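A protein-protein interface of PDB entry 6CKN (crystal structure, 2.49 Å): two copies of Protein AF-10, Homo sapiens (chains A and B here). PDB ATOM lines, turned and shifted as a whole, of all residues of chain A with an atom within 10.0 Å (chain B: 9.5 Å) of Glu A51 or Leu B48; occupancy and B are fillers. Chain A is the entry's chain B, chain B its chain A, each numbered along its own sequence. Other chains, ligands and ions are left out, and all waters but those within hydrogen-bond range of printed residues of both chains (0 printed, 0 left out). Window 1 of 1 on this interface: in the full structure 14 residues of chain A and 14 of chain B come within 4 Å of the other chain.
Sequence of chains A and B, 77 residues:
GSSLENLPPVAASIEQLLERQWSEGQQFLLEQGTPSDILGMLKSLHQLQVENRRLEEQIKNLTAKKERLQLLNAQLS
The side-chain carboxylate (OE1) of Glu B51 lies close to the side-chain amide oxygen (OE1) of Gln A47 (2.9 Å).
NH2 of Arg B54 lies within hydrogen-bond range of OG of Ser A44.
The side-chain hydroxyl of Ser B44 sits at hydrogen-bond distance from the side-chain amide oxygen of Gln A58.
Ser A44 touches Arg B54, but with the chains exchanged Arg A54 does not touch Ser B44 (4.5 Å).
Leu B48 touches its own counterpart, Leu A48.
Leu A48 touches Asn B52, and with the chains exchanged Asn A52 touches Leu B48.
Glu A51 touches Leu B48, but with the chains exchanged Leu A48 does not touch Glu B51 (4.1 Å).
14 positions are printed for both chains.
Of the 18 pairs that touch across the chains among the printed residues, 9 have their exchanged pair printed and touching as well.
Printed residues of chain B within 4 Å of Glu A51: Gln B47 and Leu B48.
No residue of chain B comes within 4 Å of Arg A54.
Of chain A, only Glu A51 (3.4 Å) comes within 4 Å of Gln B47.
Printed residues of chain A within 4 Å of Met B41: Leu A55 (3.5 Å), Gln A58 (3.7 Å) and Ile A59 (3.997 Å).
Printed residues of chain B within 4 Å of Gln A58: Gly B40 (3.8 Å), Met B41 (3.7 Å) and Ser B44 (2.7 Å).
Of the printed residues of chain A, Gly B40 touches Gln A58 (3.8 Å).
Leu B42 touches none of the printed residues of chain A.
Arg A53 touches none of the printed residues of chain B.
The nearest printed residue of chain B that does not touch Glu A51 is Ser B44 (4.1 Å).
The nearest printed residue of chain A that does not touch Leu B48 is Gln A49 (5.6 Å).
CD2 of Leu B55 touches CA of Leu A45 (3.8 Å).
OE1 of Gln A47 touches NH2 of Arg B54, at 3.6 Å.
Leu A48 touches Leu B48.
Glu A51 touches Gln B47.
CD1 of Leu B48 touches N of Asn A52, at 3.7 Å.
Met B41 touches Leu A55 (O to CD1, 3.5 Å).
Leu A55 touches Leu B45 (CD2 to CA, 3.9 Å).
CD2 of Leu A55 touches CD2 of Leu B48 (3.7 Å).
Gln A58 touches Met B41 (OE1 to CA, 3.7 Å).
CG of Met B41 touches CG1 of Ile A59 (3.997 Å).
Of the 19 printed residues of chain A, 9 touch a printed residue of chain B.
Hydrophobic or aromatic side chains of chain A that line the printed part of chain B: Leu A45, Leu A48, Leu A55 and Ile A59.
Of the 18 printed residues of chain B, 10 touch a printed residue of chain A.
Among the printed residues, 18 pairs touch across the chains.
Among the printed residues, no Asp or Glu carboxylate lies within 4 Å of a Lys or Arg side-chain nitrogen of the other chain.
OE2 of Glu A56 lies within hydrogen-bond range of ND2 of Asn A52.
OE2 of Glu B56 sits at hydrogen-bond distance from ND2 of Asn B52, at 3.2 Å.
The side-chain carboxylate (OE1) of Glu B51 lies within salt-bridge range of the guanidinium group (NH2) of Arg B54.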
ATOM      1  N   GLU A  15       7.843 -19.767   3.783  1.00  0.00           N
ATOM      2  CA  GLU A  15       7.287 -19.320   5.071  1.00  0.00           C
ATOM      3  C   GLU A  15       7.833 -20.223   6.215  1.00  0.00           C
ATOM      4  O   GLU A  15       8.101 -19.732   7.327  1.00  0.00           O
ATOM      5  CB  GLU A  15       5.735 -19.315   5.044  1.00  0.00           C
ATOM      6  CG  GLU A  15       5.053 -18.695   6.269  1.00  0.00           C
ATOM      7  CD  GLU A  15       5.393 -17.257   6.629  1.00  0.00           C
ATOM      8  N   GLU A  19      10.307 -19.223   9.351  1.00  0.00           N
ATOM      9  CA  GLU A  19       9.940 -19.671  10.695  1.00  0.00           C
ATOM     10  C   GLU A  19      11.061 -20.479  11.354  1.00  0.00           C
ATOM     11  O   GLU A  19      11.370 -20.237  12.516  1.00  0.00           O
ATOM     12  CB  GLU A  19       8.610 -20.449  10.681  1.00  0.00           C
ATOM     13  CG  GLU A  19       8.009 -20.656  12.072  1.00  0.00           C
ATOM     14  CD  GLU A  19       7.606 -19.420  12.863  1.00  0.00           C
ATOM     15  OE1 GLU A  19       7.667 -19.461  14.116  1.00  0.00           O
ATOM     16  OE2 GLU A  19       7.227 -18.408  12.226  1.00  0.00           O
ATOM     17  N   LYS A  43      10.331 -11.518  19.923  1.00  0.00           N
ATOM     18  CA  LYS A  43       9.114 -12.300  19.709  1.00  0.00           C
ATOM     19  C   LYS A  43       8.047 -11.348  19.083  1.00  0.00           C
ATOM     20  O   LYS A  43       7.459 -11.706  18.073  1.00  0.00           O
ATOM     21  CB  LYS A  43       8.626 -12.909  21.041  1.00  0.00           C
ATOM     22  CG  LYS A  43       7.558 -13.982  20.905  1.00  0.00           C
ATOM     23  N   SER A  44       7.877 -10.124  19.625  1.00  0.00           N
ATOM     24  CA  SER A  44       6.944  -9.118  19.093  1.00  0.00           C
ATOM     25  C   SER A  44       7.279  -8.679  17.665  1.00  0.00           C
ATOM     26  O   SER A  44       6.354  -8.442  16.872  1.00  0.00           O
ATOM     27  CB  SER A  44       6.891  -7.880  19.986  1.00  0.00           C
ATOM     28  OG  SER A  44       6.151  -8.096  21.174  1.00  0.00           O
ATOM     29  N   LEU A  45       8.577  -8.550  17.332  1.00  0.00           N
ATOM     30  CA  LEU A  45       8.964  -8.146  15.980  1.00  0.00           C
ATOM     31  C   LEU A  45       8.638  -9.283  14.997  1.00  0.00           C
ATOM     32  O   LEU A  45       8.161  -9.022  13.889  1.00  0.00           O
ATOM     33  CB  LEU A  45      10.453  -7.753  15.930  1.00  0.00           C
ATOM     34  CG  LEU A  45      11.062  -7.450  14.551  1.00  0.00           C
ATOM     35  CD1 LEU A  45      10.416  -6.220  13.887  1.00  0.00           C
ATOM     36  CD2 LEU A  45      12.570  -7.340  14.641  1.00  0.00           C
ATOM     37  N   HIS A  46       8.857 -10.549  15.426  1.00  0.00           N
ATOM     38  CA  HIS A  46       8.563 -11.723  14.606  1.00  0.00           C
ATOM     39  C   HIS A  46       7.066 -11.820  14.313  1.00  0.00           C
ATOM     40  O   HIS A  46       6.696 -11.957  13.143  1.00  0.00           O
ATOM     41  CB  HIS A  46       9.078 -13.002  15.270  1.00  0.00           C
ATOM     42  CG  HIS A  46       8.790 -14.247  14.494  1.00  0.00           C
ATOM     43  ND1 HIS A  46       9.348 -14.466  13.238  1.00  0.00           N
ATOM     44  CD2 HIS A  46       8.030 -15.315  14.830  1.00  0.00           C
ATOM     45  CE1 HIS A  46       8.908 -15.654  12.858  1.00  0.00           C
ATOM     46  NE2 HIS A  46       8.125 -16.210  13.791  1.00  0.00           N
ATOM     47  N   GLN A  47       6.217 -11.713  15.367  1.00  0.00           N
ATOM     48  CA  GLN A  47       4.756 -11.722  15.268  1.00  0.00           C
ATOM     49  C   GLN A  47       4.307 -10.574  14.364  1.00  0.00           C
ATOM     50  O   GLN A  47       3.478 -10.798  13.486  1.00  0.00           O
ATOM     51  CB  GLN A  47       4.111 -11.639  16.648  1.00  0.00           C
ATOM     52  CG  GLN A  47       4.171 -12.958  17.434  1.00  0.00           C
ATOM     53  CD  GLN A  47       3.954 -12.831  18.940  1.00  0.00           C
ATOM     54  OE1 GLN A  47       3.584 -11.780  19.483  1.00  0.00           O
ATOM     55  NE2 GLN A  47       4.172 -13.925  19.656  1.00  0.00           N
ATOM     56  N   LEU A  48       4.953  -9.387  14.483  1.00  0.00           N
ATOM     57  CA  LEU A  48       4.688  -8.248  13.594  1.00  0.00           C
ATOM     58  C   LEU A  48       4.945  -8.633  12.125  1.00  0.00           C
ATOM     59  O   LEU A  48       4.132  -8.305  11.252  1.00  0.00           O
ATOM     60  CB  LEU A  48       5.534  -7.011  13.988  1.00  0.00           C
ATOM     61  CG  LEU A  48       5.341  -5.716  13.150  1.00  0.00           C
ATOM     62  CD1 LEU A  48       4.040  -5.040  13.469  1.00  0.00           C
ATOM     63  CD2 LEU A  48       6.436  -4.720  13.430  1.00  0.00           C
ATOM     64  N   GLN A  49       6.065  -9.340  11.868  1.00  0.00           N
ATOM     65  CA  GLN A  49       6.486  -9.781  10.533  1.00  0.00           C
ATOM     66  C   GLN A  49       5.542 -10.836   9.930  1.00  0.00           C
ATOM     67  O   GLN A  49       5.210 -10.739   8.748  1.00  0.00           O
ATOM     68  CB  GLN A  49       7.964 -10.245  10.542  1.00  0.00           C
ATOM     69  CG  GLN A  49       8.947  -9.098  10.811  1.00  0.00           C
ATOM     70  CD  GLN A  49      10.402  -9.419  10.583  1.00  0.00           C
ATOM     71  OE1 GLN A  49      11.008 -10.263  11.269  1.00  0.00           O
ATOM     72  NE2 GLN A  49      11.022  -8.655   9.684  1.00  0.00           N
ATOM     73  N   VAL A  50       5.090 -11.817  10.746  1.00  0.00           N
ATOM     74  CA  VAL A  50       4.143 -12.880  10.383  1.00  0.00           C
ATOM     75  C   VAL A  50       2.748 -12.240  10.085  1.00  0.00           C
ATOM     76  O   VAL A  50       2.093 -12.593   9.098  1.00  0.00           O
ATOM     77  CB  VAL A  50       4.074 -13.944  11.517  1.00  0.00           C
ATOM     78  CG1 VAL A  50       2.891 -14.890  11.333  1.00  0.00           C
ATOM     79  CG2 VAL A  50       5.379 -14.727  11.636  1.00  0.00           C
ATOM     80  N   GLU A  51       2.312 -11.287  10.924  1.00  0.00           N
ATOM     81  CA  GLU A  51       1.047 -10.593  10.684  1.00  0.00           C
ATOM     82  C   GLU A  51       1.120  -9.825   9.377  1.00  0.00           C
ATOM     83  O   GLU A  51       0.151  -9.844   8.626  1.00  0.00           O
ATOM     84  CB  GLU A  51       0.677  -9.617  11.816  1.00  0.00           C
ATOM     85  CG  GLU A  51       0.253 -10.247  13.129  1.00  0.00           C
ATOM     86  CD  GLU A  51      -0.733 -11.389  13.055  1.00  0.00           C
ATOM     87  OE1 GLU A  51      -1.788 -11.249  12.390  1.00  0.00           O
ATOM     88  OE2 GLU A  51      -0.433 -12.436  13.673  1.00  0.00           O
ATOM     89  N   ASN A  52       2.268  -9.148   9.103  1.00  0.00           N
ATOM     90  CA  ASN A  52       2.434  -8.355   7.887  1.00  0.00           C
ATOM     91  C   ASN A  52       2.334  -9.240   6.651  1.00  0.00           C
ATOM     92  O   ASN A  52       1.622  -8.885   5.714  1.00  0.00           O
ATOM     93  CB  ASN A  52       3.701  -7.499   7.923  1.00  0.00           C
ATOM     94  CG  ASN A  52       3.905  -6.684   6.665  1.00  0.00           C
ATOM     95  OD1 ASN A  52       3.300  -5.635   6.476  1.00  0.00           O
ATOM     96  ND2 ASN A  52       4.742  -7.165   5.757  1.00  0.00           N
ATOM     97  N   ARG A  53       2.960 -10.436   6.708  1.00  0.00           N
ATOM     98  CA  ARG A  53       2.931 -11.425   5.640  1.00  0.00           C
ATOM     99  C   ARG A  53       1.501 -11.970   5.410  1.00  0.00           C
ATOM    100  O   ARG A  53       1.083 -12.008   4.253  1.00  0.00           O
ATOM    101  CB  ARG A  53       3.985 -12.543   5.849  1.00  0.00           C
ATOM    102  CG  ARG A  53       5.384 -12.133   5.370  1.00  0.00           C
ATOM    103  CD  ARG A  53       6.454 -13.242   5.334  1.00  0.00           C
ATOM    104  NE  ARG A  53       6.830 -13.780   6.653  1.00  0.00           N
ATOM    105  CZ  ARG A  53       7.748 -13.250   7.471  1.00  0.00           C
ATOM    106  NH1 ARG A  53       8.387 -12.132   7.133  1.00  0.00           N
ATOM    107  NH2 ARG A  53       8.024 -13.832   8.634  1.00  0.00           N
ATOM    108  N   ARG A  54       0.735 -12.331   6.486  1.00  0.00           N
ATOM    109  CA  ARG A  54      -0.656 -12.799   6.311  1.00  0.00           C
ATOM    110  C   ARG A  54      -1.568 -11.689   5.764  1.00  0.00           C
ATOM    111  O   ARG A  54      -2.376 -11.958   4.886  1.00  0.00           O
ATOM    112  CB  ARG A  54      -1.251 -13.436   7.577  1.00  0.00           C
ATOM    113  N   LEU A  55      -1.369 -10.448   6.187  1.00  0.00           N
ATOM    114  CA  LEU A  55      -2.147  -9.297   5.737  1.00  0.00           C
ATOM    115  C   LEU A  55      -1.885  -8.933   4.291  1.00  0.00           C
ATOM    116  O   LEU A  55      -2.837  -8.650   3.572  1.00  0.00           O
ATOM    117  CB  LEU A  55      -1.930  -8.089   6.673  1.00  0.00           C
ATOM    118  CG  LEU A  55      -2.602  -6.756   6.322  1.00  0.00           C
ATOM    119  CD1 LEU A  55      -4.115  -6.887   6.229  1.00  0.00           C
ATOM    120  CD2 LEU A  55      -2.220  -5.700   7.337  1.00  0.00           C
ATOM    121  N   GLU A  56      -0.619  -8.962   3.850  1.00  0.00           N
ATOM    122  CA  GLU A  56      -0.237  -8.699   2.460  1.00  0.00           C
ATOM    123  C   GLU A  56      -0.926  -9.720   1.546  1.00  0.00           C
ATOM    124  O   GLU A  56      -1.409  -9.346   0.478  1.00  0.00           O
ATOM    125  CB  GLU A  56       1.295  -8.777   2.283  1.00  0.00           C
ATOM    126  CG  GLU A  56       2.045  -7.539   2.759  1.00  0.00           C
ATOM    127  CD  GLU A  56       3.536  -7.458   2.466  1.00  0.00           C
ATOM    128  OE1 GLU A  56       4.114  -8.464   2.003  1.00  0.00           O
ATOM    129  OE2 GLU A  56       4.131  -6.379   2.693  1.00  0.00           O
ATOM    130  N   GLU A  57      -1.007 -10.994   1.987  1.00  0.00           N
ATOM    131  CA  GLU A  57      -1.615 -12.073   1.207  1.00  0.00           C
ATOM    132  C   GLU A  57      -3.128 -11.925   1.166  1.00  0.00           C
ATOM    133  O   GLU A  57      -3.739 -12.120   0.110  1.00  0.00           O
ATOM    134  CB  GLU A  57      -1.173 -13.472   1.705  1.00  0.00           C
ATOM    135  N   GLN A  58      -3.729 -11.536   2.289  1.00  0.00           N
ATOM    136  CA  GLN A  58      -5.172 -11.311   2.357  1.00  0.00           C
ATOM    137  C   GLN A  58      -5.614 -10.192   1.427  1.00  0.00           C
ATOM    138  O   GLN A  58      -6.575 -10.392   0.680  1.00  0.00           O
ATOM    139  CB  GLN A  58      -5.613 -11.085   3.788  1.00  0.00           C
ATOM    140  CG  GLN A  58      -5.645 -12.385   4.586  1.00  0.00           C
ATOM    141  CD  GLN A  58      -5.819 -12.121   6.046  1.00  0.00           C
ATOM    142  OE1 GLN A  58      -5.364 -11.116   6.563  1.00  0.00           O
ATOM    143  NE2 GLN A  58      -6.475 -13.012   6.747  1.00  0.00           N
ATOM    144  N   ILE A  59      -4.836  -9.071   1.382  1.00  0.00           N
ATOM    145  CA  ILE A  59      -5.037  -7.919   0.477  1.00  0.00           C
ATOM    146  C   ILE A  59      -4.881  -8.335  -0.992  1.00  0.00           C
ATOM    147  O   ILE A  59      -5.696  -7.957  -1.844  1.00  0.00           O
ATOM    148  CB  ILE A  59      -4.098  -6.741   0.825  1.00  0.00           C
ATOM    149  CG1 ILE A  59      -4.395  -6.199   2.241  1.00  0.00           C
ATOM    150  CG2 ILE A  59      -4.201  -5.625  -0.246  1.00  0.00           C
ATOM    151  CD1 ILE A  59      -3.333  -5.253   2.815  1.00  0.00           C
ATOM    152  N   TRP B  22     -12.143  -0.851  18.348  1.00  0.00           N
ATOM    153  CA  TRP B  22     -11.954  -1.797  17.271  1.00  0.00           C
ATOM    154  C   TRP B  22     -13.055  -2.844  17.207  1.00  0.00           C
ATOM    155  O   TRP B  22     -13.605  -3.071  16.121  1.00  0.00           O
ATOM    156  CB  TRP B  22     -10.558  -2.445  17.298  1.00  0.00           C
ATOM    157  CG  TRP B  22     -10.390  -3.367  16.133  1.00  0.00           C
ATOM    158  CD1 TRP B  22     -10.159  -3.009  14.835  1.00  0.00           C
ATOM    159  CD2 TRP B  22     -10.719  -4.759  16.111  1.00  0.00           C
ATOM    160  NE1 TRP B  22     -10.270  -4.107  14.011  1.00  0.00           N
ATOM    161  CE2 TRP B  22     -10.623  -5.194  14.769  1.00  0.00           C
ATOM    162  CE3 TRP B  22     -11.065  -5.693  17.100  1.00  0.00           C
ATOM    163  CZ2 TRP B  22     -10.804  -6.531  14.407  1.00  0.00           C
ATOM    164  CZ3 TRP B  22     -11.280  -7.005  16.733  1.00  0.00           C
ATOM    165  CH2 TRP B  22     -11.162  -7.413  15.399  1.00  0.00           C
ATOM    166  N   GLY B  40     -11.720 -10.759   7.930  1.00  0.00           N
ATOM    167  CA  GLY B  40     -10.486 -11.486   8.207  1.00  0.00           C
ATOM    168  C   GLY B  40      -9.290 -10.586   8.010  1.00  0.00           C
ATOM    169  O   GLY B  40      -8.422 -10.503   8.884  1.00  0.00           O
ATOM    170  N   MET B  41      -9.293  -9.833   6.903  1.00  0.00           N
ATOM    171  CA  MET B  41      -8.249  -8.872   6.554  1.00  0.00           C
ATOM    172  C   MET B  41      -8.110  -7.779   7.635  1.00  0.00           C
ATOM    173  O   MET B  41      -6.997  -7.467   8.062  1.00  0.00           O
ATOM    174  CB  MET B  41      -8.528  -8.273   5.167  1.00  0.00           C
ATOM    175  CG  MET B  41      -7.357  -7.487   4.595  1.00  0.00           C
ATOM    176  SD  MET B  41      -7.526  -5.608   5.082  1.00  0.00           S
ATOM    177  CE  MET B  41      -8.819  -5.082   3.698  1.00  0.00           C
ATOM    178  N   LEU B  42      -9.244  -7.236   8.100  1.00  0.00           N
ATOM    179  CA  LEU B  42      -9.320  -6.225   9.149  1.00  0.00           C
ATOM    180  C   LEU B  42      -8.872  -6.758  10.505  1.00  0.00           C
ATOM    181  O   LEU B  42      -8.287  -6.009  11.277  1.00  0.00           O
ATOM    182  CB  LEU B  42     -10.730  -5.601   9.196  1.00  0.00           C
ATOM    183  CG  LEU B  42     -11.124  -4.792   7.961  1.00  0.00           C
ATOM    184  CD1 LEU B  42     -12.568  -4.422   8.000  1.00  0.00           C
ATOM    185  CD2 LEU B  42     -10.197  -3.573   7.748  1.00  0.00           C
ATOM    186  N   LYS B  43      -9.112  -8.036  10.790  1.00  0.00           N
ATOM    187  CA  LYS B  43      -8.632  -8.704  12.006  1.00  0.00           C
ATOM    188  C   LYS B  43      -7.072  -8.704  11.956  1.00  0.00           C
ATOM    189  O   LYS B  43      -6.443  -8.287  12.925  1.00  0.00           O
ATOM    190  CB  LYS B  43      -9.190 -10.145  12.096  1.00  0.00           C
ATOM    191  CG  LYS B  43      -8.990 -10.824  13.447  1.00  0.00           C
ATOM    192  CD  LYS B  43      -9.314 -12.312  13.393  1.00  0.00           C
ATOM    193  N   SER B  44      -6.471  -9.066  10.801  1.00  0.00           N
ATOM    194  CA  SER B  44      -5.011  -9.061  10.597  1.00  0.00           C
ATOM    195  C   SER B  44      -4.396  -7.673  10.746  1.00  0.00           C
ATOM    196  O   SER B  44      -3.278  -7.570  11.249  1.00  0.00           O
ATOM    197  CB  SER B  44      -4.630  -9.622   9.224  1.00  0.00           C
ATOM    198  OG  SER B  44      -4.730 -11.032   9.193  1.00  0.00           O
ATOM    199  N   LEU B  45      -5.076  -6.622  10.265  1.00  0.00           N
ATOM    200  CA  LEU B  45      -4.553  -5.251  10.375  1.00  0.00           C
ATOM    201  C   LEU B  45      -4.544  -4.829  11.839  1.00  0.00           C
ATOM    202  O   LEU B  45      -3.578  -4.205  12.292  1.00  0.00           O
ATOM    203  CB  LEU B  45      -5.366  -4.263   9.508  1.00  0.00           C
ATOM    204  CG  LEU B  45      -5.008  -2.790   9.586  1.00  0.00           C
ATOM    205  CD1 LEU B  45      -3.590  -2.524   9.088  1.00  0.00           C
ATOM    206  CD2 LEU B  45      -6.037  -1.950   8.865  1.00  0.00           C
ATOM    207  N   HIS B  46      -5.606  -5.229  12.583  1.00  0.00           N
ATOM    208  CA  HIS B  46      -5.754  -4.987  14.011  1.00  0.00           C
ATOM    209  C   HIS B  46      -4.633  -5.693  14.779  1.00  0.00           C
ATOM    210  O   HIS B  46      -3.941  -5.045  15.548  1.00  0.00           O
ATOM    211  CB  HIS B  46      -7.118  -5.438  14.503  1.00  0.00           C
ATOM    212  CG  HIS B  46      -7.299  -5.213  15.962  1.00  0.00           C
ATOM    213  ND1 HIS B  46      -7.214  -3.940  16.514  1.00  0.00           N
ATOM    214  CD2 HIS B  46      -7.535  -6.106  16.948  1.00  0.00           C
ATOM    215  CE1 HIS B  46      -7.420  -4.102  17.808  1.00  0.00           C
ATOM    216  NE2 HIS B  46      -7.630  -5.386  18.112  1.00  0.00           N
ATOM    217  N   GLN B  47      -4.418  -6.991  14.531  1.00  0.00           N
ATOM    218  CA  GLN B  47      -3.345  -7.770  15.145  1.00  0.00           C
ATOM    219  C   GLN B  47      -2.004  -7.087  14.849  1.00  0.00           C
ATOM    220  O   GLN B  47      -1.221  -6.888  15.767  1.00  0.00           O
ATOM    221  CB  GLN B  47      -3.364  -9.204  14.601  1.00  0.00           C
ATOM    222  CG  GLN B  47      -4.603 -10.024  14.986  1.00  0.00           C
ATOM    223  CD  GLN B  47      -4.639 -11.368  14.290  1.00  0.00           C
ATOM    224  N   LEU B  48      -1.787  -6.635  13.592  1.00  0.00           N
ATOM    225  CA  LEU B  48      -0.572  -5.934  13.151  1.00  0.00           C
ATOM    226  C   LEU B  48      -0.333  -4.663  13.973  1.00  0.00           C
ATOM    227  O   LEU B  48       0.799  -4.409  14.382  1.00  0.00           O
ATOM    228  CB  LEU B  48      -0.642  -5.601  11.639  1.00  0.00           C
ATOM    229  CG  LEU B  48       0.587  -4.906  11.012  1.00  0.00           C
ATOM    230  CD1 LEU B  48       1.726  -5.897  10.810  1.00  0.00           C
ATOM    231  CD2 LEU B  48       0.259  -4.278   9.674  1.00  0.00           C
ATOM    232  N   GLN B  49      -1.407  -3.883  14.215  1.00  0.00           N
ATOM    233  CA  GLN B  49      -1.382  -2.627  14.959  1.00  0.00           C
ATOM    234  C   GLN B  49      -1.093  -2.841  16.451  1.00  0.00           C
ATOM    235  O   GLN B  49      -0.326  -2.071  17.041  1.00  0.00           O
ATOM    236  CB  GLN B  49      -2.686  -1.818  14.735  1.00  0.00           C
ATOM    237  CG  GLN B  49      -2.792  -1.282  13.305  1.00  0.00           C
ATOM    238  CD  GLN B  49      -3.884  -0.267  13.086  1.00  0.00           C
ATOM    239  OE1 GLN B  49      -5.081  -0.530  13.260  1.00  0.00           O
ATOM    240  NE2 GLN B  49      -3.494   0.887  12.591  1.00  0.00           N
ATOM    241  N   VAL B  50      -1.716  -3.889  17.039  1.00  0.00           N
ATOM    242  CA  VAL B  50      -1.553  -4.347  18.419  1.00  0.00           C
ATOM    243  C   VAL B  50      -0.060  -4.781  18.663  1.00  0.00           C
ATOM    244  O   VAL B  50       0.549  -4.358  19.656  1.00  0.00           O
ATOM    245  CB  VAL B  50      -2.595  -5.459  18.746  1.00  0.00           C
ATOM    246  CG1 VAL B  50      -2.188  -6.304  19.954  1.00  0.00           C
ATOM    247  CG2 VAL B  50      -3.980  -4.854  18.951  1.00  0.00           C
ATOM    248  N   GLU B  51       0.513  -5.575  17.729  1.00  0.00           N
ATOM    249  CA  GLU B  51       1.907  -6.015  17.768  1.00  0.00           C
ATOM    250  C   GLU B  51       2.843  -4.820  17.652  1.00  0.00           C
ATOM    251  O   GLU B  51       3.845  -4.779  18.364  1.00  0.00           O
ATOM    252  CB  GLU B  51       2.216  -7.025  16.632  1.00  0.00           C
ATOM    253  CG  GLU B  51       1.590  -8.398  16.801  1.00  0.00           C
ATOM    254  CD  GLU B  51       1.863  -9.073  18.128  1.00  0.00           C
ATOM    255  OE1 GLU B  51       3.049  -9.137  18.519  1.00  0.00           O
ATOM    256  OE2 GLU B  51       0.897  -9.518  18.787  1.00  0.00           O
ATOM    257  N   ASN B  52       2.529  -3.857  16.733  1.00  0.00           N
ATOM    258  CA  ASN B  52       3.374  -2.683  16.535  1.00  0.00           C
ATOM    259  C   ASN B  52       3.425  -1.829  17.803  1.00  0.00           C
ATOM    260  O   ASN B  52       4.505  -1.425  18.214  1.00  0.00           O
ATOM    261  CB  ASN B  52       2.968  -1.887  15.302  1.00  0.00           C
ATOM    262  CG  ASN B  52       3.841  -0.663  15.084  1.00  0.00           C
ATOM    263  OD1 ASN B  52       4.989  -0.743  14.625  1.00  0.00           O
ATOM    264  ND2 ASN B  52       3.337   0.501  15.452  1.00  0.00           N
ATOM    265  N   ARG B  53       2.277  -1.635  18.458  1.00  0.00           N
ATOM    266  CA  ARG B  53       2.151  -0.876  19.689  1.00  0.00           C
ATOM    267  C   ARG B  53       2.950  -1.517  20.843  1.00  0.00           C
ATOM    268  O   ARG B  53       3.704  -0.801  21.521  1.00  0.00           O
ATOM    269  CB  ARG B  53       0.668  -0.627  20.039  1.00  0.00           C
ATOM    270  CG  ARG B  53       0.469   0.161  21.327  1.00  0.00           C
ATOM    271  CD  ARG B  53      -0.786   1.014  21.328  1.00  0.00           C
ATOM    272  NE  ARG B  53      -0.560   2.255  22.075  1.00  0.00           N
ATOM    273  CZ  ARG B  53      -0.699   2.379  23.391  1.00  0.00           C
ATOM    274  NH1 ARG B  53      -0.441   3.533  23.983  1.00  0.00           N
ATOM    275  NH2 ARG B  53      -1.104   1.350  24.126  1.00  0.00           N
ATOM    276  N   ARG B  54       2.822  -2.844  21.042  1.00  0.00           N
ATOM    277  CA  ARG B  54       3.574  -3.561  22.080  1.00  0.00           C
ATOM    278  C   ARG B  54       5.077  -3.495  21.812  1.00  0.00           C
ATOM    279  O   ARG B  54       5.838  -3.249  22.737  1.00  0.00           O
ATOM    280  CB  ARG B  54       3.132  -5.018  22.203  1.00  0.00           C
ATOM    281  CG  ARG B  54       3.470  -5.600  23.576  1.00  0.00           C
ATOM    282  CD  ARG B  54       3.411  -7.113  23.611  1.00  0.00           C
ATOM    283  NE  ARG B  54       2.157  -7.616  23.046  1.00  0.00           N
ATOM    284  CZ  ARG B  54       2.072  -8.313  21.917  1.00  0.00           C
ATOM    285  NH1 ARG B  54       0.891  -8.723  21.473  1.00  0.00           N
ATOM    286  NH2 ARG B  54       3.168  -8.610  21.228  1.00  0.00           N
ATOM    287  N   LEU B  55       5.492  -3.673  20.548  1.00  0.00           N
ATOM    288  CA  LEU B  55       6.897  -3.595  20.160  1.00  0.00           C
ATOM    289  C   LEU B  55       7.477  -2.214  20.394  1.00  0.00           C
ATOM    290  O   LEU B  55       8.590  -2.119  20.895  1.00  0.00           O
ATOM    291  CB  LEU B  55       7.102  -4.065  18.707  1.00  0.00           C
ATOM    292  CG  LEU B  55       8.512  -3.964  18.096  1.00  0.00           C
ATOM    293  CD1 LEU B  55       9.524  -4.750  18.887  1.00  0.00           C
ATOM    294  CD2 LEU B  55       8.502  -4.430  16.668  1.00  0.00           C
ATOM    295  N   GLU B  56       6.725  -1.151  20.069  1.00  0.00           N
ATOM    296  CA  GLU B  56       7.150   0.233  20.296  1.00  0.00           C
ATOM    297  C   GLU B  56       7.388   0.464  21.795  1.00  0.00           C
ATOM    298  O   GLU B  56       8.373   1.113  22.172  1.00  0.00           O
ATOM    299  CB  GLU B  56       6.101   1.230  19.754  1.00  0.00           C
ATOM    300  CG  GLU B  56       6.144   1.409  18.239  1.00  0.00           C
ATOM    301  CD  GLU B  56       5.286   2.491  17.608  1.00  0.00           C
ATOM    302  OE1 GLU B  56       4.424   3.064  18.316  1.00  0.00           O
ATOM    303  OE2 GLU B  56       5.473   2.760  16.397  1.00  0.00           O
